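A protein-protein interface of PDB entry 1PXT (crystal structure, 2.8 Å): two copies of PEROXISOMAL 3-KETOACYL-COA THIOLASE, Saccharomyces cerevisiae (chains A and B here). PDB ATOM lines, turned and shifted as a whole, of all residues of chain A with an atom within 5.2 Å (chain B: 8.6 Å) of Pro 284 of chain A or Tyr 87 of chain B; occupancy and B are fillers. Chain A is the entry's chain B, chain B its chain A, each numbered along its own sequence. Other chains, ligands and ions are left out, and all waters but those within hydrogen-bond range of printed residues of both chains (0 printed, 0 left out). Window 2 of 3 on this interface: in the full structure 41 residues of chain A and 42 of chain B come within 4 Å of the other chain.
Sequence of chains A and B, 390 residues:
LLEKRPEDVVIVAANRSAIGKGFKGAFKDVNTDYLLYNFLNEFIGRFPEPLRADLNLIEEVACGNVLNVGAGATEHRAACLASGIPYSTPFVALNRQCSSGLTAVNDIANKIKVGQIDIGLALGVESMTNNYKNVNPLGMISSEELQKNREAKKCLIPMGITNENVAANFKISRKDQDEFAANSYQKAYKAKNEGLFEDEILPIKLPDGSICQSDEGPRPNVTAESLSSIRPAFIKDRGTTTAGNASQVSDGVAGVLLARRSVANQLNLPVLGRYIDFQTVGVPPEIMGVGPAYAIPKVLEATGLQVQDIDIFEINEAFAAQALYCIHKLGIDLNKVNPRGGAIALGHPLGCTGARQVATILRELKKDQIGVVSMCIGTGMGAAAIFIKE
NH2 of Arg 77 of chain B is in hydrogen-bond range of O of Gly 380 of chain A (3.5 Å).
O of Ser 88 of chain B sits at hydrogen-bond distance from N of Gly 282 of chain A (3.0 Å).
The guanidinium group of Arg 77 of chain B lies within hydrogen-bond range of the backbone carbonyl oxygen of Tyr 87 of chain B (3.0 Å).
NH1 of Arg 77 of chain B lies within hydrogen-bond range of O of Thr 89 of chain B.
O of Gly 380 of chain A sits at hydrogen-bond distance from N of Val 283 of chain A, 2.7 Å away.
Tyr 87 of chain B touches Gly 282 of chain A.
Val 283 of chain A touches Tyr 87 of chain B.
Pro 284 of chain A touches Tyr 87 of chain B.
CG of Pro 285 of chain A touches CD1 of Leu 81 of chain B, 3.95 Å away.
Printed residues of chain B within 4 Å of Pro 284 of chain A: Tyr 87.
Tyr 87 of chain B touches just these residues of chain A: Gly 282, Val 283 and Pro 284.
Of chain B, only Tyr 87 (3.0 Å) and Ser 88 (3.0 Å) come within 4 Å of Gly 282 of chain A.
Pro 285 of chain A touches one residue of chain B.
Printed residues of chain A within 4 Å of Arg 77 of chain B: Gly 380 (3.5 Å).
Printed residues of chain A within 4 Å of Leu 81 of chain B: Pro 285 (3.95 Å).
The nearest residue of chain B that does not touch Pro 284 of chain A is Arg 77 of chain B (6.0 Å).
The nearest residue of chain A that does not touch Tyr 87 of chain B is Pro 285 of chain A (4.1 Å).
The nearest printed residue of chain A that does not touch Arg 77 of chain B is Val 283 of chain A (4.1 Å).
Along chain A the printed residues that touch a printed residue of chain B span positions 282 to 380.
Of the 15 printed residues of chain B, 4 touch a printed residue of chain A.
Hydrophobic or aromatic side chains of chain B within 4 Å of the printed part of chain A: Leu 81 and Tyr 87.
Along chain B the printed residues that touch a printed residue of chain A span positions 77 to 88.
Among the printed residues, 6 pairs touch across the chains.
Among the printed residues, no Asp or Glu carboxylate lies within 4 Å of a Lys or Arg side-chain nitrogen of the other chain.
No position is printed for both chains.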
ATOM      1  N   GLY A 282      -5.359 -26.390  19.152  1.00  0.00           N
ATOM      2  CA  GLY A 282      -6.776 -26.268  18.893  1.00  0.00           C
ATOM      3  C   GLY A 282      -7.396 -26.864  20.132  1.00  0.00           C
ATOM      4  O   GLY A 282      -6.940 -27.910  20.640  1.00  0.00           O
ATOM      5  N   VAL A 283      -8.475 -26.222  20.564  1.00  0.00           N
ATOM      6  CA  VAL A 283      -9.214 -26.552  21.779  1.00  0.00           C
ATOM      7  C   VAL A 283     -10.745 -26.463  21.484  1.00  0.00           C
ATOM      8  O   VAL A 283     -11.167 -25.657  20.647  1.00  0.00           O
ATOM      9  CB  VAL A 283      -8.751 -25.529  22.891  1.00  0.00           C
ATOM     10  CG1 VAL A 283      -9.915 -24.587  23.354  1.00  0.00           C
ATOM     11  CG2 VAL A 283      -8.042 -26.254  24.023  1.00  0.00           C
ATOM     12  N   PRO A 284     -11.582 -27.330  22.118  1.00  0.00           N
ATOM     13  CA  PRO A 284     -13.030 -27.283  21.877  1.00  0.00           C
ATOM     14  C   PRO A 284     -13.495 -25.847  21.977  1.00  0.00           C
ATOM     15  O   PRO A 284     -13.231 -25.189  22.973  1.00  0.00           O
ATOM     16  CB  PRO A 284     -13.583 -28.132  23.014  1.00  0.00           C
ATOM     17  CG  PRO A 284     -12.560 -29.208  23.115  1.00  0.00           C
ATOM     18  CD  PRO A 284     -11.257 -28.417  23.068  1.00  0.00           C
ATOM     19  N   PRO A 285     -14.136 -25.320  20.933  1.00  0.00           N
ATOM     20  CA  PRO A 285     -14.615 -23.936  20.929  1.00  0.00           C
ATOM     21  C   PRO A 285     -15.561 -23.562  22.080  1.00  0.00           C
ATOM     22  O   PRO A 285     -15.563 -22.412  22.537  1.00  0.00           O
ATOM     23  CB  PRO A 285     -15.314 -23.811  19.565  1.00  0.00           C
ATOM     24  CG  PRO A 285     -14.569 -24.781  18.702  1.00  0.00           C
ATOM     25  CD  PRO A 285     -14.368 -25.967  19.624  1.00  0.00           C
ATOM     26  N   GLU A 286     -16.370 -24.511  22.541  1.00  0.00           N
ATOM     27  CA  GLU A 286     -17.323 -24.234  23.632  1.00  0.00           C
ATOM     28  C   GLU A 286     -16.612 -23.987  24.954  1.00  0.00           C
ATOM     29  O   GLU A 286     -17.173 -23.367  25.840  1.00  0.00           O
ATOM     30  CB  GLU A 286     -18.318 -25.383  23.853  1.00  0.00           C
ATOM     31  CG  GLU A 286     -18.516 -26.323  22.688  1.00  0.00           C
ATOM     32  CD  GLU A 286     -17.519 -27.460  22.671  1.00  0.00           C
ATOM     33  OE1 GLU A 286     -17.791 -28.494  23.318  1.00  0.00           O
ATOM     34  OE2 GLU A 286     -16.468 -27.330  22.005  1.00  0.00           O
ATOM     35  N   ILE A 287     -15.418 -24.551  25.103  1.00  0.00           N
ATOM     36  CA  ILE A 287     -14.625 -24.393  26.307  1.00  0.00           C
ATOM     37  C   ILE A 287     -13.260 -23.808  25.914  1.00  0.00           C
ATOM     38  O   ILE A 287     -12.190 -24.361  26.213  1.00  0.00           O
ATOM     39  CB  ILE A 287     -14.466 -25.733  27.068  1.00  0.00           C
ATOM     40  CG1 ILE A 287     -13.731 -26.767  26.208  1.00  0.00           C
ATOM     41  CG2 ILE A 287     -15.826 -26.234  27.517  1.00  0.00           C
ATOM     42  CD1 ILE A 287     -13.513 -28.129  26.922  1.00  0.00           C
ATOM     43  N   MET A 288     -13.326 -22.678  25.216  1.00  0.00           N
ATOM     44  CA  MET A 288     -12.157 -21.940  24.727  1.00  0.00           C
ATOM     45  C   MET A 288     -11.103 -21.670  25.786  1.00  0.00           C
ATOM     46  O   MET A 288      -9.926 -21.979  25.586  1.00  0.00           O
ATOM     47  CB  MET A 288     -12.622 -20.613  24.137  1.00  0.00           C
ATOM     48  CG  MET A 288     -11.666 -19.489  24.310  1.00  0.00           C
ATOM     49  SD  MET A 288     -12.500 -18.108  25.043  1.00  0.00           S
ATOM     50  CE  MET A 288     -11.382 -16.743  24.620  1.00  0.00           C
ATOM     51  N   GLY A 380     -11.718 -21.224  19.962  1.00  0.00           N
ATOM     52  CA  GLY A 380     -11.189 -22.478  20.469  1.00  0.00           C
ATOM     53  C   GLY A 380      -9.733 -22.794  20.252  1.00  0.00           C
ATOM     54  O   GLY A 380      -9.400 -23.835  19.697  1.00  0.00           O
ATOM     55  N   LEU B  55      -6.540 -36.154   8.933  1.00  0.00           N
ATOM     56  CA  LEU B  55      -7.012 -34.773   8.737  1.00  0.00           C
ATOM     57  C   LEU B  55      -6.600 -33.919   9.926  1.00  0.00           C
ATOM     58  O   LEU B  55      -6.673 -32.696   9.871  1.00  0.00           O
ATOM     59  CB  LEU B  55      -8.546 -34.729   8.518  1.00  0.00           C
ATOM     60  CG  LEU B  55      -9.167 -33.597   7.687  1.00  0.00           C
ATOM     61  CD1 LEU B  55      -8.470 -33.449   6.350  1.00  0.00           C
ATOM     62  CD2 LEU B  55     -10.630 -33.860   7.470  1.00  0.00           C
ATOM     63  N   ASN B  56      -6.112 -34.579  10.974  1.00  0.00           N
ATOM     64  CA  ASN B  56      -5.644 -33.933  12.194  1.00  0.00           C
ATOM     65  C   ASN B  56      -4.137 -33.825  12.105  1.00  0.00           C
ATOM     66  O   ASN B  56      -3.497 -33.279  12.977  1.00  0.00           O
ATOM     67  CB  ASN B  56      -6.033 -34.756  13.432  1.00  0.00           C
ATOM     68  CG  ASN B  56      -5.640 -36.223  13.318  1.00  0.00           C
ATOM     69  OD1 ASN B  56      -4.466 -36.589  13.456  1.00  0.00           O
ATOM     70  ND2 ASN B  56      -6.628 -37.073  13.043  1.00  0.00           N
ATOM     71  N   ILE B  58      -2.867 -32.240   9.929  1.00  0.00           N
ATOM     72  CA  ILE B  58      -2.721 -30.862   9.464  1.00  0.00           C
ATOM     73  C   ILE B  58      -2.649 -30.054  10.757  1.00  0.00           C
ATOM     74  O   ILE B  58      -3.602 -30.054  11.554  1.00  0.00           O
ATOM     75  CB  ILE B  58      -3.940 -30.415   8.635  1.00  0.00           C
ATOM     76  CG1 ILE B  58      -4.198 -31.431   7.555  1.00  0.00           C
ATOM     77  CG2 ILE B  58      -3.716 -29.043   8.012  1.00  0.00           C
ATOM     78  CD1 ILE B  58      -5.504 -31.233   6.901  1.00  0.00           C
ATOM     79  N   ARG B  77     -12.969 -20.087  10.178  1.00  0.00           N
ATOM     80  CA  ARG B  77     -12.549 -21.154  11.115  1.00  0.00           C
ATOM     81  C   ARG B  77     -13.690 -22.149  11.199  1.00  0.00           C
ATOM     82  O   ARG B  77     -13.449 -23.360  11.232  1.00  0.00           O
ATOM     83  CB  ARG B  77     -12.219 -20.589  12.509  1.00  0.00           C
ATOM     84  CG  ARG B  77     -12.273 -21.610  13.648  1.00  0.00           C
ATOM     85  CD  ARG B  77     -10.935 -22.170  14.115  1.00  0.00           C
ATOM     86  NE  ARG B  77     -11.195 -23.000  15.284  1.00  0.00           N
ATOM     87  CZ  ARG B  77     -10.491 -24.072  15.630  1.00  0.00           C
ATOM     88  NH1 ARG B  77      -9.457 -24.469  14.907  1.00  0.00           N
ATOM     89  NH2 ARG B  77     -10.845 -24.779  16.691  1.00  0.00           N
ATOM     90  N   CYS B  80     -13.848 -24.324   8.117  1.00  0.00           N
ATOM     91  CA  CYS B  80     -12.889 -25.418   8.316  1.00  0.00           C
ATOM     92  C   CYS B  80     -13.469 -26.420   9.329  1.00  0.00           C
ATOM     93  O   CYS B  80     -13.398 -27.635   9.138  1.00  0.00           O
ATOM     94  CB  CYS B  80     -11.549 -24.873   8.839  1.00  0.00           C
ATOM     95  SG  CYS B  80     -10.719 -23.662   7.742  1.00  0.00           S
ATOM     96  N   LEU B  81     -14.102 -25.891  10.372  1.00  0.00           N
ATOM     97  CA  LEU B  81     -14.699 -26.721  11.418  1.00  0.00           C
ATOM     98  C   LEU B  81     -15.766 -27.612  10.842  1.00  0.00           C
ATOM     99  O   LEU B  81     -15.826 -28.800  11.181  1.00  0.00           O
ATOM    100  CB  LEU B  81     -15.324 -25.862  12.538  1.00  0.00           C
ATOM    101  CG  LEU B  81     -14.399 -25.630  13.738  1.00  0.00           C
ATOM    102  CD1 LEU B  81     -14.992 -24.662  14.776  1.00  0.00           C
ATOM    103  CD2 LEU B  81     -14.090 -26.986  14.343  1.00  0.00           C
ATOM    104  N   ALA B  82     -16.562 -27.021   9.945  1.00  0.00           N
ATOM    105  CA  ALA B  82     -17.695 -27.656   9.273  1.00  0.00           C
ATOM    106  C   ALA B  82     -17.261 -28.646   8.200  1.00  0.00           C
ATOM    107  O   ALA B  82     -17.889 -29.680   8.044  1.00  0.00           O
ATOM    108  CB  ALA B  82     -18.626 -26.594   8.684  1.00  0.00           C
ATOM    109  N   GLY B  84     -15.120 -30.731   8.294  1.00  0.00           N
ATOM    110  CA  GLY B  84     -14.371 -31.801   8.931  1.00  0.00           C
ATOM    111  C   GLY B  84     -12.960 -31.579   9.450  1.00  0.00           C
ATOM    112  O   GLY B  84     -12.388 -32.515  10.026  1.00  0.00           O
ATOM    113  N   ILE B  85     -12.361 -30.404   9.243  1.00  0.00           N
ATOM    114  CA  ILE B  85     -11.004 -30.175   9.770  1.00  0.00           C
ATOM    115  C   ILE B  85     -11.231 -30.012  11.265  1.00  0.00           C
ATOM    116  O   ILE B  85     -12.064 -29.216  11.669  1.00  0.00           O
ATOM    117  CB  ILE B  85     -10.336 -28.923   9.152  1.00  0.00           C
ATOM    118  CG1 ILE B  85     -10.261 -29.095   7.621  1.00  0.00           C
ATOM    119  CG2 ILE B  85      -8.939 -28.750   9.721  1.00  0.00           C
ATOM    120  CD1 ILE B  85      -9.588 -27.976   6.896  1.00  0.00           C
ATOM    121  N   PRO B  86     -10.538 -30.808  12.094  1.00  0.00           N
ATOM    122  CA  PRO B  86     -10.656 -30.795  13.558  1.00  0.00           C
ATOM    123  C   PRO B  86     -10.347 -29.483  14.326  1.00  0.00           C
ATOM    124  O   PRO B  86      -9.603 -28.622  13.829  1.00  0.00           O
ATOM    125  CB  PRO B  86      -9.773 -31.979  13.970  1.00  0.00           C
ATOM    126  CG  PRO B  86      -8.708 -31.938  12.949  1.00  0.00           C
ATOM    127  CD  PRO B  86      -9.459 -31.717  11.671  1.00  0.00           C
ATOM    128  N   TYR B  87     -10.983 -29.324  15.506  1.00  0.00           N
ATOM    129  CA  TYR B  87     -10.795 -28.142  16.364  1.00  0.00           C
ATOM    130  C   TYR B  87      -9.338 -28.052  16.719  1.00  0.00           C
ATOM    131  O   TYR B  87      -8.780 -26.966  16.763  1.00  0.00           O
ATOM    132  CB  TYR B  87     -11.621 -28.218  17.658  1.00  0.00           C
ATOM    133  CG  TYR B  87     -11.320 -29.393  18.599  1.00  0.00           C
ATOM    134  CD1 TYR B  87     -10.125 -29.474  19.308  1.00  0.00           C
ATOM    135  CD2 TYR B  87     -12.240 -30.413  18.775  1.00  0.00           C
ATOM    136  CE1 TYR B  87      -9.856 -30.538  20.155  1.00  0.00           C
ATOM    137  CE2 TYR B  87     -11.986 -31.476  19.617  1.00  0.00           C
ATOM    138  CZ  TYR B  87     -10.790 -31.542  20.306  1.00  0.00           C
ATOM    139  OH  TYR B  87     -10.535 -32.637  21.127  1.00  0.00           O
ATOM    140  N   SER B  88      -8.735 -29.231  16.888  1.00  0.00           N
ATOM    141  CA  SER B  88      -7.326 -29.418  17.235  1.00  0.00           C
ATOM    142  C   SER B  88      -6.396 -28.596  16.349  1.00  0.00           C
ATOM    143  O   SER B  88      -5.292 -28.212  16.759  1.00  0.00           O
ATOM    144  CB  SER B  88      -6.923 -30.894  17.052  1.00  0.00           C
ATOM    145  OG  SER B  88      -7.815 -31.808  17.672  1.00  0.00           O
ATOM    146  N   THR B  89      -6.823 -28.370  15.111  1.00  0.00           N
ATOM    147  CA  THR B  89      -5.998 -27.646  14.180  1.00  0.00           C
ATOM    148  C   THR B  89      -6.158 -26.174  14.356  1.00  0.00           C
ATOM    149  O   THR B  89      -7.267 -25.673  14.292  1.00  0.00           O
ATOM    150  CB  THR B  89      -6.358 -28.003  12.746  1.00  0.00           C
ATOM    151  OG1 THR B  89      -6.050 -29.388  12.495  1.00  0.00           O
ATOM    152  CG2 THR B  89      -5.612 -27.139  11.785  1.00  0.00           C
ATOM    153  N   PRO B  90      -5.087 -25.483  14.767  1.00  0.00           N
ATOM    154  CA  PRO B  90      -5.155 -24.027  14.937  1.00  0.00           C
ATOM    155  C   PRO B  90      -5.486 -23.431  13.586  1.00  0.00           C
ATOM    156  O   PRO B  90      -5.402 -24.131  12.574  1.00  0.00           O
ATOM    157  CB  PRO B  90      -3.730 -23.656  15.368  1.00  0.00           C
ATOM    158  CG  PRO B  90      -2.920 -24.830  15.015  1.00  0.00           C
ATOM    159  CD  PRO B  90      -3.829 -25.991  15.326  1.00  0.00           C
ATOM    160  N   PHE B  91      -5.686 -22.116  13.551  1.00  0.00           N
ATOM    161  CA  PHE B  91      -6.064 -21.391  12.334  1.00  0.00           C
ATOM    162  C   PHE B  91      -5.519 -19.963  12.459  1.00  0.00           C
ATOM    163  O   PHE B  91      -5.439 -19.446  13.559  1.00  0.00           O
ATOM    164  CB  PHE B  91      -7.612 -21.393  12.262  1.00  0.00           C
ATOM    165  CG  PHE B  91      -8.192 -20.553  11.162  1.00  0.00           C
ATOM    166  CD1 PHE B  91      -8.309 -19.182  11.307  1.00  0.00           C
ATOM    167  CD2 PHE B  91      -8.598 -21.129   9.973  1.00  0.00           C
ATOM    168  CE1 PHE B  91      -8.812 -18.399  10.270  1.00  0.00           C
ATOM    169  CE2 PHE B  91      -9.098 -20.354   8.940  1.00  0.00           C
ATOM    170  CZ  PHE B  91      -9.204 -18.998   9.087  1.00  0.00           C
